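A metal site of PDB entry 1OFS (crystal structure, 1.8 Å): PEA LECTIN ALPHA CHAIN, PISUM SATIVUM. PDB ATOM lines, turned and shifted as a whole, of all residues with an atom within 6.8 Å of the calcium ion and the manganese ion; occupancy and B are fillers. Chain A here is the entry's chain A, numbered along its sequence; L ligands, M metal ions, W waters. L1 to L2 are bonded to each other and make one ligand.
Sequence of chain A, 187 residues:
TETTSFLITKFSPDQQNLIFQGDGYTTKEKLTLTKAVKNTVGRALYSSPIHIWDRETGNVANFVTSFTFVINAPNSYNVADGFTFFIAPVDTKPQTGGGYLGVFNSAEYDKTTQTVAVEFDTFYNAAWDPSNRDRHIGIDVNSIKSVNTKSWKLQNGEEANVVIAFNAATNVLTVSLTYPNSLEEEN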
ATOM      1  N   ASP A  81     -12.295  23.756 -11.916  1.00  0.00           N
ATOM      2  CA  ASP A  81     -11.054  23.064 -11.588  1.00  0.00           C
ATOM      3  C   ASP A  81     -10.164  23.952 -10.739  1.00  0.00           C
ATOM      4  O   ASP A  81      -9.312  23.479  -9.999  1.00  0.00           O
ATOM      5  CB  ASP A  81     -10.279  22.697 -12.847  1.00  0.00           C
ATOM      6  CG  ASP A  81     -10.516  21.271 -13.256  1.00  0.00           C
ATOM      7  OD1 ASP A  81     -11.277  21.061 -14.221  1.00  0.00           O
ATOM      8  OD2 ASP A  81     -10.005  20.313 -12.653  1.00  0.00           O
ATOM      9  N   GLY A  98      -8.997  22.033 -18.037  1.00  0.00           N
ATOM     10  CA  GLY A  98      -9.337  21.086 -16.998  1.00  0.00           C
ATOM     11  C   GLY A  98      -8.375  21.206 -15.828  1.00  0.00           C
ATOM     12  O   GLY A  98      -8.032  22.312 -15.377  1.00  0.00           O
ATOM     13  N   GLY A  99      -7.906  20.055 -15.346  1.00  0.00           N
ATOM     14  CA  GLY A  99      -6.992  19.995 -14.219  1.00  0.00           C
ATOM     15  C   GLY A  99      -5.647  20.671 -14.426  1.00  0.00           C
ATOM     16  O   GLY A  99      -4.901  20.837 -13.467  1.00  0.00           O
ATOM     17  N   TYR A 100      -5.330  21.035 -15.670  1.00  0.00           N
ATOM     18  CA  TYR A 100      -4.071  21.717 -15.973  1.00  0.00           C
ATOM     19  C   TYR A 100      -4.154  23.236 -15.802  1.00  0.00           C
ATOM     20  O   TYR A 100      -3.177  23.946 -16.000  1.00  0.00           O
ATOM     21  CB  TYR A 100      -3.550  21.332 -17.358  1.00  0.00           C
ATOM     22  CG  TYR A 100      -3.145  19.871 -17.438  1.00  0.00           C
ATOM     23  CD1 TYR A 100      -4.039  18.907 -17.889  1.00  0.00           C
ATOM     24  CD2 TYR A 100      -1.879  19.453 -17.031  1.00  0.00           C
ATOM     25  CE1 TYR A 100      -3.679  17.569 -17.959  1.00  0.00           C
ATOM     26  CE2 TYR A 100      -1.511  18.115 -17.085  1.00  0.00           C
ATOM     27  CZ  TYR A 100      -2.416  17.180 -17.563  1.00  0.00           C
ATOM     28  OH  TYR A 100      -2.078  15.846 -17.625  1.00  0.00           O
ATOM     29  N   LEU A 101      -5.348  23.723 -15.452  1.00  0.00           N
ATOM     30  CA  LEU A 101      -5.608  25.143 -15.149  1.00  0.00           C
ATOM     31  C   LEU A 101      -5.247  26.180 -16.206  1.00  0.00           C
ATOM     32  O   LEU A 101      -5.129  27.373 -15.898  1.00  0.00           O
ATOM     33  CB  LEU A 101      -4.957  25.508 -13.796  1.00  0.00           C
ATOM     34  CG  LEU A 101      -5.395  24.575 -12.653  1.00  0.00           C
ATOM     35  CD1 LEU A 101      -4.650  24.848 -11.340  1.00  0.00           C
ATOM     36  CD2 LEU A 101      -6.896  24.739 -12.449  1.00  0.00           C
ATOM     37  N   GLU A 119      -1.609  28.425  -7.678  1.00  0.00           N
ATOM     38  CA  GLU A 119      -2.918  27.826  -7.916  1.00  0.00           C
ATOM     39  C   GLU A 119      -3.819  27.725  -6.698  1.00  0.00           C
ATOM     40  O   GLU A 119      -3.350  27.596  -5.567  1.00  0.00           O
ATOM     41  CB  GLU A 119      -2.754  26.409  -8.507  1.00  0.00           C
ATOM     42  CG  GLU A 119      -2.086  25.414  -7.552  1.00  0.00           C
ATOM     43  CD  GLU A 119      -2.156  23.982  -8.062  1.00  0.00           C
ATOM     44  OE1 GLU A 119      -2.558  23.091  -7.297  1.00  0.00           O
ATOM     45  OE2 GLU A 119      -1.813  23.748  -9.246  1.00  0.00           O
ATOM     46  N   ASP A 121      -6.551  25.362  -6.327  1.00  0.00           N
ATOM     47  CA  ASP A 121      -7.031  24.109  -6.899  1.00  0.00           C
ATOM     48  C   ASP A 121      -8.223  23.527  -6.163  1.00  0.00           C
ATOM     49  O   ASP A 121      -8.096  23.112  -5.020  1.00  0.00           O
ATOM     50  CB  ASP A 121      -5.832  23.133  -6.866  1.00  0.00           C
ATOM     51  CG  ASP A 121      -6.020  21.940  -7.754  1.00  0.00           C
ATOM     52  OD1 ASP A 121      -7.176  21.636  -8.105  1.00  0.00           O
ATOM     53  OD2 ASP A 121      -5.059  21.206  -8.133  1.00  0.00           O
ATOM     54  N   THR A 122      -9.367  23.442  -6.831  1.00  0.00           N
ATOM     55  CA  THR A 122     -10.595  22.959  -6.207  1.00  0.00           C
ATOM     56  C   THR A 122     -10.978  21.510  -6.490  1.00  0.00           C
ATOM     57  O   THR A 122     -11.987  21.023  -5.985  1.00  0.00           O
ATOM     58  CB  THR A 122     -11.791  23.833  -6.649  1.00  0.00           C
ATOM     59  OG1 THR A 122     -11.840  23.877  -8.077  1.00  0.00           O
ATOM     60  CG2 THR A 122     -11.608  25.286  -6.218  1.00  0.00           C
ATOM     61  N   PHE A 123     -10.199  20.829  -7.326  1.00  0.00           N
ATOM     62  CA  PHE A 123     -10.525  19.445  -7.692  1.00  0.00           C
ATOM     63  C   PHE A 123      -9.324  18.513  -7.590  1.00  0.00           C
ATOM     64  O   PHE A 123      -8.242  18.801  -8.091  1.00  0.00           O
ATOM     65  CB  PHE A 123     -11.110  19.417  -9.114  1.00  0.00           C
ATOM     66  CG  PHE A 123     -11.450  18.036  -9.601  1.00  0.00           C
ATOM     67  CD1 PHE A 123     -12.699  17.483  -9.362  1.00  0.00           C
ATOM     68  CD2 PHE A 123     -10.519  17.281 -10.303  1.00  0.00           C
ATOM     69  CE1 PHE A 123     -13.012  16.209  -9.815  1.00  0.00           C
ATOM     70  CE2 PHE A 123     -10.822  16.017 -10.762  1.00  0.00           C
ATOM     71  CZ  PHE A 123     -12.074  15.477 -10.522  1.00  0.00           C
ATOM     72  N   TYR A 124      -9.528  17.359  -6.959  1.00  0.00           N
ATOM     73  CA  TYR A 124      -8.447  16.384  -6.789  1.00  0.00           C
ATOM     74  C   TYR A 124      -8.146  15.588  -8.056  1.00  0.00           C
ATOM     75  O   TYR A 124      -8.966  14.767  -8.496  1.00  0.00           O
ATOM     76  CB  TYR A 124      -8.762  15.421  -5.630  1.00  0.00           C
ATOM     77  CG  TYR A 124      -7.850  14.205  -5.549  1.00  0.00           C
ATOM     78  CD1 TYR A 124      -6.490  14.350  -5.285  1.00  0.00           C
ATOM     79  CD2 TYR A 124      -8.350  12.931  -5.718  1.00  0.00           C
ATOM     80  CE1 TYR A 124      -5.660  13.232  -5.204  1.00  0.00           C
ATOM     81  CE2 TYR A 124      -7.530  11.812  -5.638  1.00  0.00           C
ATOM     82  CZ  TYR A 124      -6.192  11.976  -5.380  1.00  0.00           C
ATOM     83  OH  TYR A 124      -5.372  10.857  -5.300  1.00  0.00           O
ATOM     84  N   ASN A 125      -6.984  15.829  -8.637  1.00  0.00           N
ATOM     85  CA  ASN A 125      -6.515  15.100  -9.804  1.00  0.00           C
ATOM     86  C   ASN A 125      -5.541  14.079  -9.223  1.00  0.00           C
ATOM     87  O   ASN A 125      -4.420  14.412  -8.850  1.00  0.00           O
ATOM     88  CB  ASN A 125      -5.812  16.029 -10.801  1.00  0.00           C
ATOM     89  CG  ASN A 125      -6.756  17.013 -11.463  1.00  0.00           C
ATOM     90  OD1 ASN A 125      -6.870  18.160 -11.048  1.00  0.00           O
ATOM     91  ND2 ASN A 125      -7.444  16.556 -12.515  1.00  0.00           N
ATOM     92  N   TRP A 128      -1.539  13.687  -9.717  1.00  0.00           N
ATOM     93  CA  TRP A 128      -0.530  14.569  -9.170  1.00  0.00           C
ATOM     94  C   TRP A 128      -0.883  15.398  -7.937  1.00  0.00           C
ATOM     95  O   TRP A 128       0.012  15.888  -7.258  1.00  0.00           O
ATOM     96  CB  TRP A 128      -0.035  15.512 -10.274  1.00  0.00           C
ATOM     97  CG  TRP A 128      -1.125  16.386 -10.804  1.00  0.00           C
ATOM     98  CD1 TRP A 128      -1.677  17.474 -10.185  1.00  0.00           C
ATOM     99  CD2 TRP A 128      -1.797  16.237 -12.050  1.00  0.00           C
ATOM    100  NE1 TRP A 128      -2.663  18.008 -10.982  1.00  0.00           N
ATOM    101  CE2 TRP A 128      -2.760  17.281 -12.129  1.00  0.00           C
ATOM    102  CE3 TRP A 128      -1.687  15.341 -13.122  1.00  0.00           C
ATOM    103  CZ2 TRP A 128      -3.595  17.434 -13.230  1.00  0.00           C
ATOM    104  CZ3 TRP A 128      -2.524  15.499 -14.200  1.00  0.00           C
ATOM    105  CH2 TRP A 128      -3.467  16.537 -14.258  1.00  0.00           C
ATOM    106  N   ASP A 129      -2.179  15.578  -7.652  1.00  0.00           N
ATOM    107  CA  ASP A 129      -2.577  16.396  -6.508  1.00  0.00           C
ATOM    108  C   ASP A 129      -2.318  15.705  -5.161  1.00  0.00           C
ATOM    109  O   ASP A 129      -2.159  14.482  -5.119  1.00  0.00           O
ATOM    110  CB  ASP A 129      -4.050  16.818  -6.624  1.00  0.00           C
ATOM    111  CG  ASP A 129      -4.254  17.984  -7.585  1.00  0.00           C
ATOM    112  OD1 ASP A 129      -3.326  18.823  -7.700  1.00  0.00           O
ATOM    113  OD2 ASP A 129      -5.283  18.136  -8.259  1.00  0.00           O
ATOM    114  N   PRO A 130      -2.243  16.487  -4.086  1.00  0.00           N
ATOM    115  CA  PRO A 130      -1.988  15.926  -2.754  1.00  0.00           C
ATOM    116  C   PRO A 130      -2.951  14.769  -2.439  1.00  0.00           C
ATOM    117  O   PRO A 130      -4.155  14.894  -2.626  1.00  0.00           O
ATOM    118  CB  PRO A 130      -2.226  17.121  -1.827  1.00  0.00           C
ATOM    119  CG  PRO A 130      -1.871  18.295  -2.685  1.00  0.00           C
ATOM    120  CD  PRO A 130      -2.383  17.949  -4.059  1.00  0.00           C
ATOM    121  N   HIS A 136      -6.662  22.837  -2.413  1.00  0.00           N
ATOM    122  CA  HIS A 136      -5.420  23.372  -1.900  1.00  0.00           C
ATOM    123  C   HIS A 136      -4.844  24.517  -2.702  1.00  0.00           C
ATOM    124  O   HIS A 136      -5.177  24.715  -3.869  1.00  0.00           O
ATOM    125  CB  HIS A 136      -4.371  22.251  -1.953  1.00  0.00           C
ATOM    126  CG  HIS A 136      -4.292  21.572  -3.295  1.00  0.00           C
ATOM    127  ND1 HIS A 136      -5.154  20.561  -3.665  1.00  0.00           N
ATOM    128  CD2 HIS A 136      -3.473  21.784  -4.355  1.00  0.00           C
ATOM    129  CE1 HIS A 136      -4.872  20.173  -4.889  1.00  0.00           C
ATOM    130  NE2 HIS A 136      -3.853  20.899  -5.340  1.00  0.00           N
ATOM    131  N   ILE A 137      -3.979  25.285  -2.044  1.00  0.00           N
ATOM    132  CA  ILE A 137      -3.252  26.359  -2.676  1.00  0.00           C
ATOM    133  C   ILE A 137      -1.920  25.717  -3.023  1.00  0.00           C
ATOM    134  O   ILE A 137      -1.420  24.871  -2.266  1.00  0.00           O
ATOM    135  CB  ILE A 137      -3.036  27.534  -1.718  1.00  0.00           C
ATOM    136  CG1 ILE A 137      -4.385  28.099  -1.259  1.00  0.00           C
ATOM    137  CG2 ILE A 137      -2.199  28.641  -2.399  1.00  0.00           C
ATOM    138  CD1 ILE A 137      -4.270  29.109  -0.131  1.00  0.00           C
ATOM    139  N   GLY A 138      -1.336  26.072  -4.157  1.00  0.00           N
ATOM    140  CA  GLY A 138      -0.059  25.483  -4.529  1.00  0.00           C
ATOM    141  C   GLY A 138       0.833  26.419  -5.297  1.00  0.00           C
ATOM    142  O   GLY A 138       0.368  27.402  -5.874  1.00  0.00           O
ATOM    143  N   ASP A 140       3.343  26.372  -8.385  1.00  0.00           N
ATOM    144  CA  ASP A 140       3.680  25.557  -9.553  1.00  0.00           C
ATOM    145  C   ASP A 140       4.847  26.118 -10.328  1.00  0.00           C
ATOM    146  O   ASP A 140       4.850  27.306 -10.679  1.00  0.00           O
ATOM    147  CB  ASP A 140       2.479  25.493 -10.506  1.00  0.00           C
ATOM    148  CG  ASP A 140       1.241  24.914  -9.857  1.00  0.00           C
ATOM    149  OD1 ASP A 140       1.353  24.371  -8.729  1.00  0.00           O
ATOM    150  OD2 ASP A 140       0.119  24.935 -10.414  1.00  0.00           O
ATOM    151  N   ILE A 144       2.214  21.105 -13.456  1.00  0.00           N
ATOM    152  CA  ILE A 144       0.967  21.164 -12.690  1.00  0.00           C
ATOM    153  C   ILE A 144       1.113  20.480 -11.326  1.00  0.00           C
ATOM    154  O   ILE A 144       0.280  20.648 -10.432  1.00  0.00           O
ATOM    155  CB  ILE A 144      -0.192  20.578 -13.512  1.00  0.00           C
ATOM    156  CG1 ILE A 144      -1.547  20.947 -12.896  1.00  0.00           C
ATOM    157  CG2 ILE A 144      -0.030  19.065 -13.650  1.00  0.00           C
ATOM    158  CD1 ILE A 144      -1.884  22.426 -12.989  1.00  0.00           C
ATOM    159  N   LYS A 145       2.182  19.705 -11.164  1.00  0.00           N
ATOM    160  CA  LYS A 145       2.470  19.060  -9.889  1.00  0.00           C
ATOM    161  C   LYS A 145       3.236  20.071  -9.053  1.00  0.00           C
ATOM    162  O   LYS A 145       4.455  20.250  -9.240  1.00  0.00           O
ATOM    163  CB  LYS A 145       3.301  17.792 -10.087  1.00  0.00           C
ATOM    164  CG  LYS A 145       3.522  17.024  -8.800  1.00  0.00           C
ATOM    165  CD  LYS A 145       4.511  15.872  -8.979  1.00  0.00           C
ATOM    166  CE  LYS A 145       4.748  15.133  -7.674  1.00  0.00           C
ATOM    167  NZ  LYS A 145       3.609  15.301  -6.722  1.00  0.00           N
ATOM    168  N   SER A 146       2.537  20.717  -8.125  1.00  0.00           N
ATOM    169  CA  SER A 146       3.139  21.757  -7.286  1.00  0.00           C
ATOM    170  C   SER A 146       4.392  21.364  -6.499  1.00  0.00           C
ATOM    171  O   SER A 146       4.543  20.210  -6.088  1.00  0.00           O
ATOM    172  CB  SER A 146       2.095  22.306  -6.303  1.00  0.00           C
ATOM    173  OG  SER A 146       0.811  22.448  -6.904  1.00  0.00           O
ATOM    174  N   THR A 149       2.303  22.761  -1.386  1.00  0.00           N
ATOM    175  CA  THR A 149       0.870  22.995  -1.293  1.00  0.00           C
ATOM    176  C   THR A 149       0.442  23.243   0.138  1.00  0.00           C
ATOM    177  O   THR A 149       1.202  23.033   1.080  1.00  0.00           O
ATOM    178  CB  THR A 149       0.060  21.783  -1.818  1.00  0.00           C
ATOM    179  OG1 THR A 149       0.514  20.590  -1.149  1.00  0.00           O
ATOM    180  CG2 THR A 149       0.331  21.521  -3.300  1.00  0.00           C
HETATM  181  C1  LIG L   1     -12.118  15.712 -16.206  1.00  0.00           C
HETATM  182  C2  LIG L   1     -10.895  16.408 -16.822  1.00  0.00           C
HETATM  183  C3  LIG L   1      -9.893  16.818 -15.713  1.00  0.00           C
HETATM  184  C4  LIG L   1     -10.606  17.734 -14.707  1.00  0.00           C
HETATM  185  C5  LIG L   1     -11.853  16.997 -14.139  1.00  0.00           C
HETATM  186  C6  LIG L   1     -12.723  17.814 -13.192  1.00  0.00           C
HETATM  187  O1  LIG L   1     -10.262  15.528 -17.714  1.00  0.00           O
HETATM  188  O2  LIG L   1      -8.823  17.531 -16.326  1.00  0.00           O
HETATM  189  O3  LIG L   1      -9.721  18.033 -13.628  1.00  0.00           O
HETATM  190  O4  LIG L   1     -12.738  16.631 -15.267  1.00  0.00           O
HETATM  191  O5  LIG L   1     -13.146  19.006 -13.881  1.00  0.00           O
HETATM  192  C1  LG2 L   2     -12.543  12.931 -17.179  1.00  0.00           C
HETATM  193  C2  LG2 L   2     -12.562  13.392 -15.729  1.00  0.00           C
HETATM  194  C3  LG2 L   2     -12.122  12.268 -14.769  1.00  0.00           C
HETATM  195  C4  LG2 L   2     -12.657  12.811 -13.474  1.00  0.00           C
HETATM  196  C5  LG2 L   2     -14.075  13.183 -13.957  1.00  0.00           C
HETATM  197  C6  LG2 L   2     -14.746  14.224 -13.085  1.00  0.00           C
HETATM  198  O1  LG2 L   2     -13.522  11.896 -17.378  1.00  0.00           O
HETATM  199  O2  LG2 L   2     -11.704  14.531 -15.566  1.00  0.00           O
HETATM  200  O3  LG2 L   2     -10.701  12.162 -14.721  1.00  0.00           O
HETATM  201  O4  LG2 L   2     -12.723  11.780 -12.482  1.00  0.00           O
HETATM  202  O5  LG2 L   2     -13.890  13.699 -15.318  1.00  0.00           O
HETATM  203  O6  LG2 L   2     -16.124  14.235 -13.348  1.00  0.00           O
HETATM  204 CA    CA M   1      -6.548  19.750  -9.387  1.00  0.00          CA
HETATM  205 MN    MN M   2      -3.069  20.958  -7.486  1.00  0.00          MN
HETATM  206  O   HOH W   1      -4.666  20.296 -10.860  1.00  0.00           O
HETATM  207  O   HOH W   2      -2.272  21.236  -9.586  1.00  0.00           O
HETATM  208  O   HOH W   3      -8.038  20.931 -10.819  1.00  0.00           O
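The calcium ion is bound by the side-chain amide oxygen (OD1) of Asn 125, 2.3 Å away. O of Phe 123 binds the calcium ion, at 2.3 Å. OD2 of Asp 129 is bound to the calcium ion, 2.3 Å away. The side-chain carboxylate (OD1) of Asp 121 binds the calcium ion (2.4 Å). Water W3 binds the calcium ion (2.4 Å). OD2 of Asp 121 binds the calcium ion, 2.4 Å away. Water W1 binds the calcium ion.
Four residues have an atom within 4 Å of the calcium ion: Asp 121, Phe 123, Asn 125 and Asp 129.
The manganese ion is bound by the side-chain carboxylate (OD2) of Asp 121 (2.1 Å), the side-chain carboxylate (OD1) of Asp 129 (2.2 Å), the side-chain carboxylate (OE1) of Glu 119 (2.2 Å), water W2 (2.3 Å) and a ring nitrogen (NE2) of His 136 (2.3 Å). The manganese ion has five donor atoms within binding distance.
Water W1 bridges O of Gly 99 (2.7 Å) and NE1 of Trp 128 (3.0 Å). Water W2 bridges OE2 of Glu 119 (2.6 Å) and O of Ile 144 (2.8 Å).
O of Gly 138 sits at hydrogen-bond distance from N of Glu 119. NE1 of Trp 128 sits close to OD1 of Asp 129, at 3.4 Å. OE2 of Glu 119 lies close to OD2 of Asp 140 (2.6 Å). OG of Ser 146 sits close to OE1 of Glu 119, at 3.5 Å.
Four residues have an atom within 4 Å of the manganese ion: Glu 119, Asp 121, Asp 129 and His 136. The nearest printed residue that does not touch the manganese ion is Ser 146 (4.2 Å).
The backbone NH of Gly 99 lies within hydrogen-bond range of an oxygen (O2) of LIG L1, 2.9 Å away. The side-chain carboxylate of Asp 81 is in hydrogen-bond range of an oxygen (O3) of LIG L1. The side-chain amide nitrogen of Asn 125 is in hydrogen-bond range of an oxygen (O3) of LIG L1 (2.9 Å).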
